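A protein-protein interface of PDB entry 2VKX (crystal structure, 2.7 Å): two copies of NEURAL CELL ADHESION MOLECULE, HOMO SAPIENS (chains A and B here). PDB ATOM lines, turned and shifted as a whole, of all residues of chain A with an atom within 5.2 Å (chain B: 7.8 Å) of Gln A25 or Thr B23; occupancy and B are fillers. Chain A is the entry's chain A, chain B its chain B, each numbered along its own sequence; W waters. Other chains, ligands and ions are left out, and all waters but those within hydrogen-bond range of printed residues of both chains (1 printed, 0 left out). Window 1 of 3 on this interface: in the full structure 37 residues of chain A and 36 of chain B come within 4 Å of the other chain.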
ATOM      1  N   GLN A  16      23.181   6.381 -10.979  1.00  0.00           N
ATOM      2  CA  GLN A  16      23.962   5.343 -11.623  1.00  0.00           C
ATOM      3  C   GLN A  16      24.269   5.644 -13.067  1.00  0.00           C
ATOM      4  O   GLN A  16      23.532   6.353 -13.742  1.00  0.00           O
ATOM      5  CB  GLN A  16      23.205   4.007 -11.591  1.00  0.00           C
ATOM      6  CG  GLN A  16      22.872   3.490 -10.222  1.00  0.00           C
ATOM      7  CD  GLN A  16      24.099   3.041  -9.464  1.00  0.00           C
ATOM      8  OE1 GLN A  16      24.042   2.807  -8.263  1.00  0.00           O
ATOM      9  NE2 GLN A  16      25.217   2.912 -10.166  1.00  0.00           N
ATOM     10  N   VAL A  17      25.375   5.082 -13.529  1.00  0.00           N
ATOM     11  CA  VAL A  17      25.762   5.185 -14.922  1.00  0.00           C
ATOM     12  C   VAL A  17      26.448   3.873 -15.243  1.00  0.00           C
ATOM     13  O   VAL A  17      27.631   3.703 -14.978  1.00  0.00           O
ATOM     14  CB  VAL A  17      26.738   6.343 -15.209  1.00  0.00           C
ATOM     15  CG1 VAL A  17      27.118   6.310 -16.691  1.00  0.00           C
ATOM     16  CG2 VAL A  17      26.092   7.686 -14.873  1.00  0.00           C
ATOM     17  N   GLU A  18      25.687   2.920 -15.766  1.00  0.00           N
ATOM     18  CA  GLU A  18      26.260   1.632 -16.134  1.00  0.00           C
ATOM     19  C   GLU A  18      26.681   1.707 -17.583  1.00  0.00           C
ATOM     20  O   GLU A  18      25.843   1.711 -18.472  1.00  0.00           O
ATOM     21  CB  GLU A  18      25.250   0.494 -15.983  1.00  0.00           C
ATOM     22  CG  GLU A  18      25.709  -0.782 -16.680  1.00  0.00           C
ATOM     23  CD  GLU A  18      26.969  -1.399 -16.067  1.00  0.00           C
ATOM     24  OE1 GLU A  18      27.796  -0.669 -15.470  1.00  0.00           O
ATOM     25  OE2 GLU A  18      27.142  -2.626 -16.199  1.00  0.00           O
ATOM     26  N   PRO A  19      27.994   1.776 -17.837  1.00  0.00           N
ATOM     27  CA  PRO A  19      28.491   1.852 -19.211  1.00  0.00           C
ATOM     28  C   PRO A  19      28.660   0.494 -19.872  1.00  0.00           C
ATOM     29  O   PRO A  19      29.051  -0.481 -19.238  1.00  0.00           O
ATOM     30  CB  PRO A  19      29.815   2.570 -19.051  1.00  0.00           C
ATOM     31  CG  PRO A  19      30.313   1.986 -17.780  1.00  0.00           C
ATOM     32  CD  PRO A  19      29.092   1.981 -16.877  1.00  0.00           C
ATOM     33  N   TYR A  20      28.340   0.454 -21.156  1.00  0.00           N
ATOM     34  CA  TYR A  20      28.475  -0.736 -21.969  1.00  0.00           C
ATOM     35  C   TYR A  20      29.319  -0.285 -23.150  1.00  0.00           C
ATOM     36  O   TYR A  20      29.915   0.792 -23.117  1.00  0.00           O
ATOM     37  CB  TYR A  20      27.105  -1.230 -22.416  1.00  0.00           C
ATOM     38  CG  TYR A  20      26.311  -1.837 -21.281  1.00  0.00           C
ATOM     39  CD1 TYR A  20      24.962  -1.540 -21.107  1.00  0.00           C
ATOM     40  CD2 TYR A  20      26.918  -2.692 -20.356  1.00  0.00           C
ATOM     41  CE1 TYR A  20      24.238  -2.068 -20.037  1.00  0.00           C
ATOM     42  CE2 TYR A  20      26.202  -3.224 -19.287  1.00  0.00           C
ATOM     43  CZ  TYR A  20      24.864  -2.906 -19.131  1.00  0.00           C
ATOM     44  OH  TYR A  20      24.152  -3.398 -18.057  1.00  0.00           O
ATOM     45  N   THR A  23      26.294   1.757 -25.576  1.00  0.00           N
ATOM     46  CA  THR A  23      25.186   2.359 -24.850  1.00  0.00           C
ATOM     47  C   THR A  23      25.586   2.542 -23.397  1.00  0.00           C
ATOM     48  O   THR A  23      26.581   1.986 -22.941  1.00  0.00           O
ATOM     49  CB  THR A  23      23.937   1.494 -24.877  1.00  0.00           C
ATOM     50  OG1 THR A  23      24.197   0.267 -24.189  1.00  0.00           O
ATOM     51  CG2 THR A  23      23.530   1.205 -26.299  1.00  0.00           C
ATOM     52  N   ALA A  24      24.808   3.337 -22.681  1.00  0.00           N
ATOM     53  CA  ALA A  24      25.066   3.603 -21.276  1.00  0.00           C
ATOM     54  C   ALA A  24      23.719   3.826 -20.609  1.00  0.00           C
ATOM     55  O   ALA A  24      22.892   4.577 -21.110  1.00  0.00           O
ATOM     56  CB  ALA A  24      25.950   4.852 -21.123  1.00  0.00           C
ATOM     57  N   GLN A  25      23.484   3.161 -19.491  1.00  0.00           N
ATOM     58  CA  GLN A  25      22.222   3.335 -18.807  1.00  0.00           C
ATOM     59  C   GLN A  25      22.394   4.321 -17.671  1.00  0.00           C
ATOM     60  O   GLN A  25      23.272   4.159 -16.814  1.00  0.00           O
ATOM     61  CB  GLN A  25      21.717   2.002 -18.269  1.00  0.00           C
ATOM     62  CG  GLN A  25      21.586   0.942 -19.329  1.00  0.00           C
ATOM     63  CD  GLN A  25      20.953  -0.308 -18.794  1.00  0.00           C
ATOM     64  OE1 GLN A  25      21.192  -0.688 -17.649  1.00  0.00           O
ATOM     65  NE2 GLN A  25      20.151  -0.968 -19.620  1.00  0.00           N
ATOM     66  N   VAL A  26      21.559   5.352 -17.675  1.00  0.00           N
ATOM     67  CA  VAL A  26      21.636   6.356 -16.637  1.00  0.00           C
ATOM     68  C   VAL A  26      20.441   6.261 -15.709  1.00  0.00           C
ATOM     69  O   VAL A  26      19.294   6.382 -16.136  1.00  0.00           O
ATOM     70  CB  VAL A  26      21.736   7.758 -17.237  1.00  0.00           C
ATOM     71  CG1 VAL A  26      21.726   8.797 -16.139  1.00  0.00           C
ATOM     72  CG2 VAL A  26      23.022   7.873 -18.038  1.00  0.00           C
ATOM     73  N   GLN A  27      20.739   6.020 -14.438  1.00  0.00           N
ATOM     74  CA  GLN A  27      19.736   5.893 -13.397  1.00  0.00           C
ATOM     75  C   GLN A  27      19.724   7.226 -12.677  1.00  0.00           C
ATOM     76  O   GLN A  27      20.774   7.716 -12.276  1.00  0.00           O
ATOM     77  CB  GLN A  27      20.144   4.796 -12.424  1.00  0.00           C
ATOM     78  CG  GLN A  27      19.026   3.885 -11.982  1.00  0.00           C
ATOM     79  CD  GLN A  27      19.454   2.993 -10.843  1.00  0.00           C
ATOM     80  OE1 GLN A  27      19.571   3.444  -9.703  1.00  0.00           O
ATOM     81  NE2 GLN A  27      19.714   1.720 -11.144  1.00  0.00           N
ATOM     82  N   ILE A  69      15.402   4.434 -15.577  1.00  0.00           N
ATOM     83  CA  ILE A  69      16.558   4.730 -16.397  1.00  0.00           C
ATOM     84  C   ILE A  69      16.246   5.371 -17.741  1.00  0.00           C
ATOM     85  O   ILE A  69      15.094   5.444 -18.173  1.00  0.00           O
ATOM     86  CB  ILE A  69      17.366   3.448 -16.692  1.00  0.00           C
ATOM     87  CG1 ILE A  69      16.426   2.382 -17.273  1.00  0.00           C
ATOM     88  CG2 ILE A  69      18.085   2.976 -15.431  1.00  0.00           C
ATOM     89  CD1 ILE A  69      17.127   1.183 -17.894  1.00  0.00           C
ATOM     90  N   VAL A  70      17.307   5.835 -18.389  1.00  0.00           N
ATOM     91  CA  VAL A  70      17.247   6.421 -19.713  1.00  0.00           C
ATOM     92  C   VAL A  70      18.545   5.925 -20.332  1.00  0.00           C
ATOM     93  O   VAL A  70      19.613   6.064 -19.726  1.00  0.00           O
ATOM     94  CB  VAL A  70      17.239   7.962 -19.681  1.00  0.00           C
ATOM     95  CG1 VAL A  70      15.983   8.452 -19.018  1.00  0.00           C
ATOM     96  CG2 VAL A  70      18.465   8.479 -18.960  1.00  0.00           C
ATOM     97  N   THR A  71      18.455   5.326 -21.515  1.00  0.00           N
ATOM     98  CA  THR A  71      19.630   4.789 -22.188  1.00  0.00           C
ATOM     99  C   THR A  71      20.109   5.621 -23.365  1.00  0.00           C
ATOM    100  O   THR A  71      19.394   5.809 -24.351  1.00  0.00           O
ATOM    101  CB  THR A  71      19.377   3.356 -22.713  1.00  0.00           C
ATOM    102  OG1 THR A  71      19.079   2.486 -21.623  1.00  0.00           O
ATOM    103  CG2 THR A  71      20.600   2.828 -23.442  1.00  0.00           C
ATOM    104  N   VAL B  17      18.707  -9.391 -28.950  1.00  0.00           N
ATOM    105  CA  VAL B  17      18.327  -9.331 -27.550  1.00  0.00           C
ATOM    106  C   VAL B  17      19.638  -9.454 -26.776  1.00  0.00           C
ATOM    107  O   VAL B  17      20.247 -10.524 -26.730  1.00  0.00           O
ATOM    108  CB  VAL B  17      17.352 -10.465 -27.138  1.00  0.00           C
ATOM    109  CG1 VAL B  17      16.964 -10.297 -25.680  1.00  0.00           C
ATOM    110  CG2 VAL B  17      16.104 -10.433 -28.001  1.00  0.00           C
ATOM    111  N   GLU B  18      20.093  -8.339 -26.211  1.00  0.00           N
ATOM    112  CA  GLU B  18      21.329  -8.322 -25.430  1.00  0.00           C
ATOM    113  C   GLU B  18      20.970  -8.445 -23.961  1.00  0.00           C
ATOM    114  O   GLU B  18      20.424  -7.527 -23.369  1.00  0.00           O
ATOM    115  CB  GLU B  18      22.108  -7.023 -25.671  1.00  0.00           C
ATOM    116  CG  GLU B  18      23.353  -6.867 -24.819  1.00  0.00           C
ATOM    117  CD  GLU B  18      24.286  -8.079 -24.881  1.00  0.00           C
ATOM    118  OE1 GLU B  18      23.982  -9.048 -25.606  1.00  0.00           O
ATOM    119  OE2 GLU B  18      25.330  -8.067 -24.195  1.00  0.00           O
ATOM    120  N   PRO B  19      21.282  -9.587 -23.344  1.00  0.00           N
ATOM    121  CA  PRO B  19      20.918  -9.690 -21.934  1.00  0.00           C
ATOM    122  C   PRO B  19      21.986  -9.271 -20.932  1.00  0.00           C
ATOM    123  O   PRO B  19      23.168  -9.600 -21.070  1.00  0.00           O
ATOM    124  CB  PRO B  19      20.551 -11.167 -21.794  1.00  0.00           C
ATOM    125  CG  PRO B  19      21.593 -11.826 -22.655  1.00  0.00           C
ATOM    126  CD  PRO B  19      21.708 -10.894 -23.882  1.00  0.00           C
ATOM    127  N   TYR B  20      21.540  -8.546 -19.917  1.00  0.00           N
ATOM    128  CA  TYR B  20      22.398  -8.116 -18.835  1.00  0.00           C
ATOM    129  C   TYR B  20      21.923  -8.874 -17.591  1.00  0.00           C
ATOM    130  O   TYR B  20      21.437 -10.000 -17.712  1.00  0.00           O
ATOM    131  CB  TYR B  20      22.292  -6.605 -18.670  1.00  0.00           C
ATOM    132  CG  TYR B  20      22.882  -5.877 -19.853  1.00  0.00           C
ATOM    133  CD1 TYR B  20      22.113  -5.011 -20.631  1.00  0.00           C
ATOM    134  CD2 TYR B  20      24.205  -6.097 -20.230  1.00  0.00           C
ATOM    135  CE1 TYR B  20      22.649  -4.392 -21.752  1.00  0.00           C
ATOM    136  CE2 TYR B  20      24.743  -5.484 -21.343  1.00  0.00           C
ATOM    137  CZ  TYR B  20      23.961  -4.637 -22.098  1.00  0.00           C
ATOM    138  OH  TYR B  20      24.512  -4.043 -23.198  1.00  0.00           O
ATOM    139  N   SER B  21      22.039  -8.286 -16.405  1.00  0.00           N
ATOM    140  CA  SER B  21      21.618  -8.985 -15.196  1.00  0.00           C
ATOM    141  C   SER B  21      20.156  -8.787 -14.849  1.00  0.00           C
ATOM    142  O   SER B  21      19.470  -9.743 -14.513  1.00  0.00           O
ATOM    143  CB  SER B  21      22.484  -8.570 -14.012  1.00  0.00           C
ATOM    144  OG  SER B  21      23.828  -8.958 -14.227  1.00  0.00           O
ATOM    145  N   SER B  22      19.679  -7.553 -14.929  1.00  0.00           N
ATOM    146  CA  SER B  22      18.285  -7.254 -14.621  1.00  0.00           C
ATOM    147  C   SER B  22      17.597  -6.494 -15.764  1.00  0.00           C
ATOM    148  O   SER B  22      16.446  -6.080 -15.641  1.00  0.00           O
ATOM    149  CB  SER B  22      18.207  -6.431 -13.349  1.00  0.00           C
ATOM    150  OG  SER B  22      18.930  -5.220 -13.513  1.00  0.00           O
ATOM    151  N   THR B  23      18.315  -6.286 -16.859  1.00  0.00           N
ATOM    152  CA  THR B  23      17.753  -5.610 -18.015  1.00  0.00           C
ATOM    153  C   THR B  23      18.194  -6.364 -19.253  1.00  0.00           C
ATOM    154  O   THR B  23      19.087  -7.208 -19.193  1.00  0.00           O
ATOM    155  CB  THR B  23      18.222  -4.138 -18.150  1.00  0.00           C
ATOM    156  OG1 THR B  23      19.620  -4.092 -18.461  1.00  0.00           O
ATOM    157  CG2 THR B  23      17.961  -3.382 -16.871  1.00  0.00           C
ATOM    158  N   ALA B  24      17.546  -6.061 -20.373  1.00  0.00           N
ATOM    159  CA  ALA B  24      17.856  -6.683 -21.655  1.00  0.00           C
ATOM    160  C   ALA B  24      17.526  -5.665 -22.736  1.00  0.00           C
ATOM    161  O   ALA B  24      16.488  -5.002 -22.678  1.00  0.00           O
ATOM    162  CB  ALA B  24      17.011  -7.950 -21.842  1.00  0.00           C
ATOM    163  N   GLN B  25      18.415  -5.515 -23.706  1.00  0.00           N
ATOM    164  CA  GLN B  25      18.170  -4.581 -24.795  1.00  0.00           C
ATOM    165  C   GLN B  25      17.644  -5.359 -25.974  1.00  0.00           C
ATOM    166  O   GLN B  25      18.334  -6.234 -26.487  1.00  0.00           O
ATOM    167  CB  GLN B  25      19.447  -3.848 -25.202  1.00  0.00           C
ATOM    168  CG  GLN B  25      20.035  -3.015 -24.083  1.00  0.00           C
ATOM    169  CD  GLN B  25      21.163  -2.132 -24.547  1.00  0.00           C
ATOM    170  OE1 GLN B  25      21.881  -2.463 -25.495  1.00  0.00           O
ATOM    171  NE2 GLN B  25      21.338  -1.002 -23.873  1.00  0.00           N
ATOM    172  N   VAL B  26      16.420  -5.042 -26.390  1.00  0.00           N
ATOM    173  CA  VAL B  26      15.803  -5.710 -27.526  1.00  0.00           C
ATOM    174  C   VAL B  26      15.900  -4.812 -28.755  1.00  0.00           C
ATOM    175  O   VAL B  26      15.580  -3.620 -28.692  1.00  0.00           O
ATOM    176  CB  VAL B  26      14.290  -6.028 -27.268  1.00  0.00           C
ATOM    177  CG1 VAL B  26      13.671  -6.675 -28.497  1.00  0.00           C
ATOM    178  CG2 VAL B  26      14.127  -6.949 -26.072  1.00  0.00           C
ATOM    179  N   ILE B  69      16.218   0.604 -29.961  1.00  0.00           N
ATOM    180  CA  ILE B  69      15.978  -0.473 -29.024  1.00  0.00           C
ATOM    181  C   ILE B  69      14.936  -0.092 -27.987  1.00  0.00           C
ATOM    182  O   ILE B  69      14.530   1.065 -27.876  1.00  0.00           O
ATOM    183  CB  ILE B  69      17.270  -0.850 -28.225  1.00  0.00           C
ATOM    184  CG1 ILE B  69      17.801   0.382 -27.496  1.00  0.00           C
ATOM    185  CG2 ILE B  69      18.334  -1.425 -29.143  1.00  0.00           C
ATOM    186  CD1 ILE B  69      19.041   0.117 -26.684  1.00  0.00           C
ATOM    187  N   THR B  71      14.297  -1.265 -23.869  1.00  0.00           N
ATOM    188  CA  THR B  71      14.937  -1.962 -22.780  1.00  0.00           C
ATOM    189  C   THR B  71      13.936  -2.438 -21.741  1.00  0.00           C
ATOM    190  O   THR B  71      13.225  -1.636 -21.137  1.00  0.00           O
ATOM    191  CB  THR B  71      15.990  -1.041 -22.123  1.00  0.00           C
ATOM    192  OG1 THR B  71      16.930  -0.620 -23.121  1.00  0.00           O
ATOM    193  CG2 THR B  71      16.731  -1.769 -20.997  1.00  0.00           C
ATOM    194  N   ILE B  72      13.872  -3.752 -21.556  1.00  0.00           N
ATOM    195  CA  ILE B  72      12.978  -4.330 -20.572  1.00  0.00           C
ATOM    196  C   ILE B  72      13.778  -4.305 -19.278  1.00  0.00           C
ATOM    197  O   ILE B  72      14.977  -4.589 -19.274  1.00  0.00           O
ATOM    198  CB  ILE B  72      12.590  -5.768 -20.941  1.00  0.00           C
ATOM    199  CG1 ILE B  72      13.840  -6.610 -21.124  1.00  0.00           C
ATOM    200  CG2 ILE B  72      11.834  -5.788 -22.255  1.00  0.00           C
ATOM    201  CD1 ILE B  72      13.533  -8.044 -21.437  1.00  0.00           C
ATOM    202  N   VAL B  73      13.119  -3.936 -18.185  1.00  0.00           N
ATOM    203  CA  VAL B  73      13.774  -3.834 -16.893  1.00  0.00           C
ATOM    204  C   VAL B  73      13.080  -4.695 -15.845  1.00  0.00           C
ATOM    205  O   VAL B  73      12.043  -5.310 -16.123  1.00  0.00           O
ATOM    206  CB  VAL B  73      13.797  -2.359 -16.413  1.00  0.00           C
ATOM    207  CG1 VAL B  73      14.520  -1.490 -17.435  1.00  0.00           C
ATOM    208  CG2 VAL B  73      12.384  -1.852 -16.222  1.00  0.00           C
ATOM    209  N   GLY B  74      13.667  -4.744 -14.649  1.00  0.00           N
ATOM    210  CA  GLY B  74      13.096  -5.519 -13.563  1.00  0.00           C
ATOM    211  C   GLY B  74      13.197  -7.023 -13.719  1.00  0.00           C
ATOM    212  O   GLY B  74      12.344  -7.757 -13.233  1.00  0.00           O
ATOM    213  N   LEU B  75      14.240  -7.492 -14.390  1.00  0.00           N
ATOM    214  CA  LEU B  75      14.433  -8.927 -14.589  1.00  0.00           C
ATOM    215  C   LEU B  75      15.286  -9.496 -13.457  1.00  0.00           C
ATOM    216  O   LEU B  75      15.944  -8.755 -12.737  1.00  0.00           O
ATOM    217  CB  LEU B  75      15.131  -9.176 -15.931  1.00  0.00           C
ATOM    218  CG  LEU B  75      14.527  -8.486 -17.157  1.00  0.00           C
ATOM    219  CD1 LEU B  75      15.457  -8.645 -18.336  1.00  0.00           C
ATOM    220  CD2 LEU B  75      13.162  -9.076 -17.475  1.00  0.00           C
ATOM    221  N   LYS B  76      15.272 -10.813 -13.301  1.00  0.00           N
ATOM    222  CA  LYS B  76      16.066 -11.473 -12.272  1.00  0.00           C
ATOM    223  C   LYS B  76      17.295 -12.059 -12.945  1.00  0.00           C
ATOM    224  O   LYS B  76      17.223 -12.521 -14.082  1.00  0.00           O
ATOM    225  CB  LYS B  76      15.277 -12.614 -11.620  1.00  0.00           C
ATOM    226  CG  LYS B  76      14.040 -12.195 -10.849  1.00  0.00           C
ATOM    227  CD  LYS B  76      13.220 -13.423 -10.482  1.00  0.00           C
ATOM    228  CE  LYS B  76      11.913 -13.058  -9.790  1.00  0.00           C
ATOM    229  NZ  LYS B  76      12.152 -12.358  -8.499  1.00  0.00           N
ATOM    230  N   PRO B  77      18.444 -12.047 -12.254  1.00  0.00           N
ATOM    231  CA  PRO B  77      19.689 -12.592 -12.809  1.00  0.00           C
ATOM    232  C   PRO B  77      19.640 -14.094 -13.060  1.00  0.00           C
ATOM    233  O   PRO B  77      18.840 -14.814 -12.468  1.00  0.00           O
ATOM    234  CB  PRO B  77      20.727 -12.225 -11.749  1.00  0.00           C
ATOM    235  CG  PRO B  77      20.198 -10.948 -11.201  1.00  0.00           C
ATOM    236  CD  PRO B  77      18.723 -11.252 -11.046  1.00  0.00           C
ATOM    237  N   TYR B  81      14.270 -16.212 -20.021  1.00  0.00           N
ATOM    238  CA  TYR B  81      13.057 -15.483 -20.341  1.00  0.00           C
ATOM    239  C   TYR B  81      12.709 -15.632 -21.810  1.00  0.00           C
ATOM    240  O   TYR B  81      13.556 -15.980 -22.647  1.00  0.00           O
ATOM    241  CB  TYR B  81      13.246 -13.992 -20.056  1.00  0.00           C
ATOM    242  CG  TYR B  81      13.313 -13.604 -18.602  1.00  0.00           C
ATOM    243  CD1 TYR B  81      12.152 -13.330 -17.874  1.00  0.00           C
ATOM    244  CD2 TYR B  81      14.540 -13.477 -17.956  1.00  0.00           C
ATOM    245  CE1 TYR B  81      12.218 -12.938 -16.540  1.00  0.00           C
ATOM    246  CE2 TYR B  81      14.619 -13.085 -16.617  1.00  0.00           C
ATOM    247  CZ  TYR B  81      13.459 -12.821 -15.920  1.00  0.00           C
ATOM    248  OH  TYR B  81      13.542 -12.473 -14.600  1.00  0.00           O
ATOM    249  N   PHE B 102      16.107 -15.975 -24.064  1.00  0.00           N
ATOM    250  CA  PHE B 102      17.419 -15.467 -23.660  1.00  0.00           C
ATOM    251  C   PHE B 102      17.670 -15.672 -22.182  1.00  0.00           C
ATOM    252  O   PHE B 102      16.741 -15.863 -21.411  1.00  0.00           O
ATOM    253  CB  PHE B 102      17.538 -13.972 -23.972  1.00  0.00           C
ATOM    254  CG  PHE B 102      16.653 -13.092 -23.117  1.00  0.00           C
ATOM    255  CD1 PHE B 102      17.065 -12.674 -21.858  1.00  0.00           C
ATOM    256  CD2 PHE B 102      15.406 -12.669 -23.585  1.00  0.00           C
ATOM    257  CE1 PHE B 102      16.254 -11.849 -21.083  1.00  0.00           C
ATOM    258  CE2 PHE B 102      14.595 -11.846 -22.816  1.00  0.00           C
ATOM    259  CZ  PHE B 102      15.020 -11.436 -21.566  1.00  0.00           C
ATOM    260  N   LYS B 103      18.933 -15.617 -21.777  1.00  0.00           N
ATOM    261  CA  LYS B 103      19.250 -15.790 -20.369  1.00  0.00           C
ATOM    262  C   LYS B 103      20.025 -14.612 -19.800  1.00  0.00           C
ATOM    263  O   LYS B 103      21.075 -14.246 -20.315  1.00  0.00           O
ATOM    264  CB  LYS B 103      20.045 -17.077 -20.146  1.00  0.00           C
ATOM    265  CG  LYS B 103      20.123 -17.456 -18.683  1.00  0.00           C
ATOM    266  CD  LYS B 103      20.932 -18.703 -18.472  1.00  0.00           C
ATOM    267  CE  LYS B 103      20.955 -19.081 -16.994  1.00  0.00           C
ATOM    268  NZ  LYS B 103      22.062 -20.036 -16.718  1.00  0.00           N
ATOM    269  N   THR B 104      19.496 -14.029 -18.729  1.00  0.00           N
ATOM    270  CA  THR B 104      20.138 -12.894 -18.075  1.00  0.00           C
ATOM    271  C   THR B 104      21.476 -13.289 -17.472  1.00  0.00           C
ATOM    272  O   THR B 104      21.672 -14.427 -17.049  1.00  0.00           O
ATOM    273  CB  THR B 104      19.262 -12.318 -16.942  1.00  0.00           C
ATOM    274  OG1 THR B 104      18.866 -13.377 -16.064  1.00  0.00           O
ATOM    275  CG2 THR B 104      18.032 -11.631 -17.511  1.00  0.00           C
ATOM    276  N   GLN B 105      22.397 -12.340 -17.426  1.00  0.00           N
ATOM    277  CA  GLN B 105      23.710 -12.604 -16.862  1.00  0.00           C
ATOM    278  C   GLN B 105      23.675 -12.663 -15.332  1.00  0.00           C
ATOM    279  O   GLN B 105      22.739 -12.176 -14.699  1.00  0.00           O
ATOM    280  CB  GLN B 105      24.697 -11.518 -17.301  1.00  0.00           C
ATOM    281  CG  GLN B 105      24.916 -11.442 -18.796  1.00  0.00           C
ATOM    282  CD  GLN B 105      26.029 -10.488 -19.163  1.00  0.00           C
ATOM    283  OE1 GLN B 105      27.137 -10.580 -18.627  1.00  0.00           O
ATOM    284  NE2 GLN B 105      25.748  -9.567 -20.088  1.00  0.00           N
ATOM    285  N   ASP B 135      29.521  -1.620 -13.330  1.00  0.00           N
ATOM    286  CA  ASP B 135      29.206  -1.869 -11.919  1.00  0.00           C
ATOM    287  C   ASP B 135      28.951  -3.339 -11.639  1.00  0.00           C
ATOM    288  O   ASP B 135      28.474  -3.692 -10.570  1.00  0.00           O
ATOM    289  CB  ASP B 135      27.971  -1.062 -11.459  1.00  0.00           C
ATOM    290  CG  ASP B 135      26.707  -1.342 -12.308  1.00  0.00           C
ATOM    291  OD1 ASP B 135      26.580  -2.442 -12.898  1.00  0.00           O
ATOM    292  OD2 ASP B 135      25.824  -0.456 -12.370  1.00  0.00           O
ATOM    293  N   GLY B 137      26.746  -5.210 -13.156  1.00  0.00           N
ATOM    294  CA  GLY B 137      25.364  -5.573 -13.394  1.00  0.00           C
ATOM    295  C   GLY B 137      24.390  -5.324 -12.265  1.00  0.00           C
ATOM    296  O   GLY B 137      23.247  -5.789 -12.314  1.00  0.00           O
HETATM  297  O   HOH W   1      19.142  -0.183 -22.107  1.00  0.00           O
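Gln A25 touches just these residues of chain B: Thr B23 (3.4 Å) and Thr B71 (3.8 Å).
Of chain A, only Gln A25 (3.4 Å) comes within 4 Å of Thr B23.
No residue of chain B comes within 4 Å of Ala A24.
Of the printed residues of chain B, Thr A71 touches Gln B25.
Printed residues of chain B within 4 Å of Glu A18: Asp B135 (2.9 Å).
Printed residues of chain A within 4 Å of Asp B135: Glu A18 (2.9 Å).
Printed residues of chain A within 4 Å of Thr B71: Gln A25.
Of the printed residues of chain B, Thr A23 touches Gln B25 (3.1 Å).
Gln A16 touches none of the printed residues of chain B.
Pro A19 touches none of the printed residues of chain B.
The nearest residue of chain B that does not touch Gln A25 is Gln B25 (4.4 Å).
The nearest residue of chain A that does not touch Thr B23 is Tyr A20 (4.6 Å).
The nearest printed residue of chain A that does not touch Tyr B20 is Thr A23 (4.4 Å).
Tyr A20 touches its own counterpart, Tyr B20.
Thr A23 touches Gln B25, and with the chains exchanged Gln A25 touches Thr B23.
Gln A25 touches Thr B71, and with the chains exchanged Thr A71 touches Gln B25.
Positions printed for both chains: 17, 18, 19, 20, 23, 24, 25, 26, 69 and 71.
Of the 7 pairs that touch across the chains among the printed residues, 5 have their exchanged pair printed and touching as well.
The side-chain hydroxyl of Thr B23 lies within hydrogen-bond range of the side-chain amide nitrogen of Gln A25, 3.4 Å away.
OE1 of Glu A18 lies within hydrogen-bond range of N of Asp B135 (2.9 Å).
The side-chain amide nitrogen (NE2) of Gln B25 sits at hydrogen-bond distance from the side-chain hydroxyl (OG1) of Thr A23.
The backbone NH (N) of Glu A18 sits at hydrogen-bond distance from the backbone carbonyl oxygen (O) of Gln A25, 2.9 Å away.
The backbone carbonyl oxygen (O) of Tyr B20 lies within hydrogen-bond range of the backbone NH (N) of Gln B105 (2.5 Å).
The side-chain carboxylate (OD1) of Asp B135 is in hydrogen-bond range of the backbone NH (N) of Gly B137, 2.8 Å away.
The backbone NH (N) of Glu B18 lies within hydrogen-bond range of the backbone carbonyl oxygen (O) of Gln B25, 2.8 Å away.
Water W1 lies within hydrogen-bond range of OG1 of Thr B71 (2.5 Å), OG1 of Thr A71 (2.7 Å), NE2 of Gln A25 (2.8 Å) and NE2 of Gln B25 (2.9 Å).
Of the 25 printed residues of chain B, 6 touch a printed residue of chain A.
Hydrophobic or aromatic side chains of chain B that line the printed part of chain A: Tyr B20 and Val B73.
Of the 13 printed residues of chain A, 6 touch a printed residue of chain B.
Among the printed residues, no Asp or Glu carboxylate lies within 4 Å of a Lys or Arg side-chain nitrogen of the other chain.
OH of Tyr B20 touches CD1 of Tyr A20, at 3.3 Å.
Gln A25 touches Thr B71 (NE2 to CG2, 3.8 Å).
CG1 of Val B73 touches CD1 of Ile A69, 3.8 Å away.
Gln B25 touches Thr A71.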
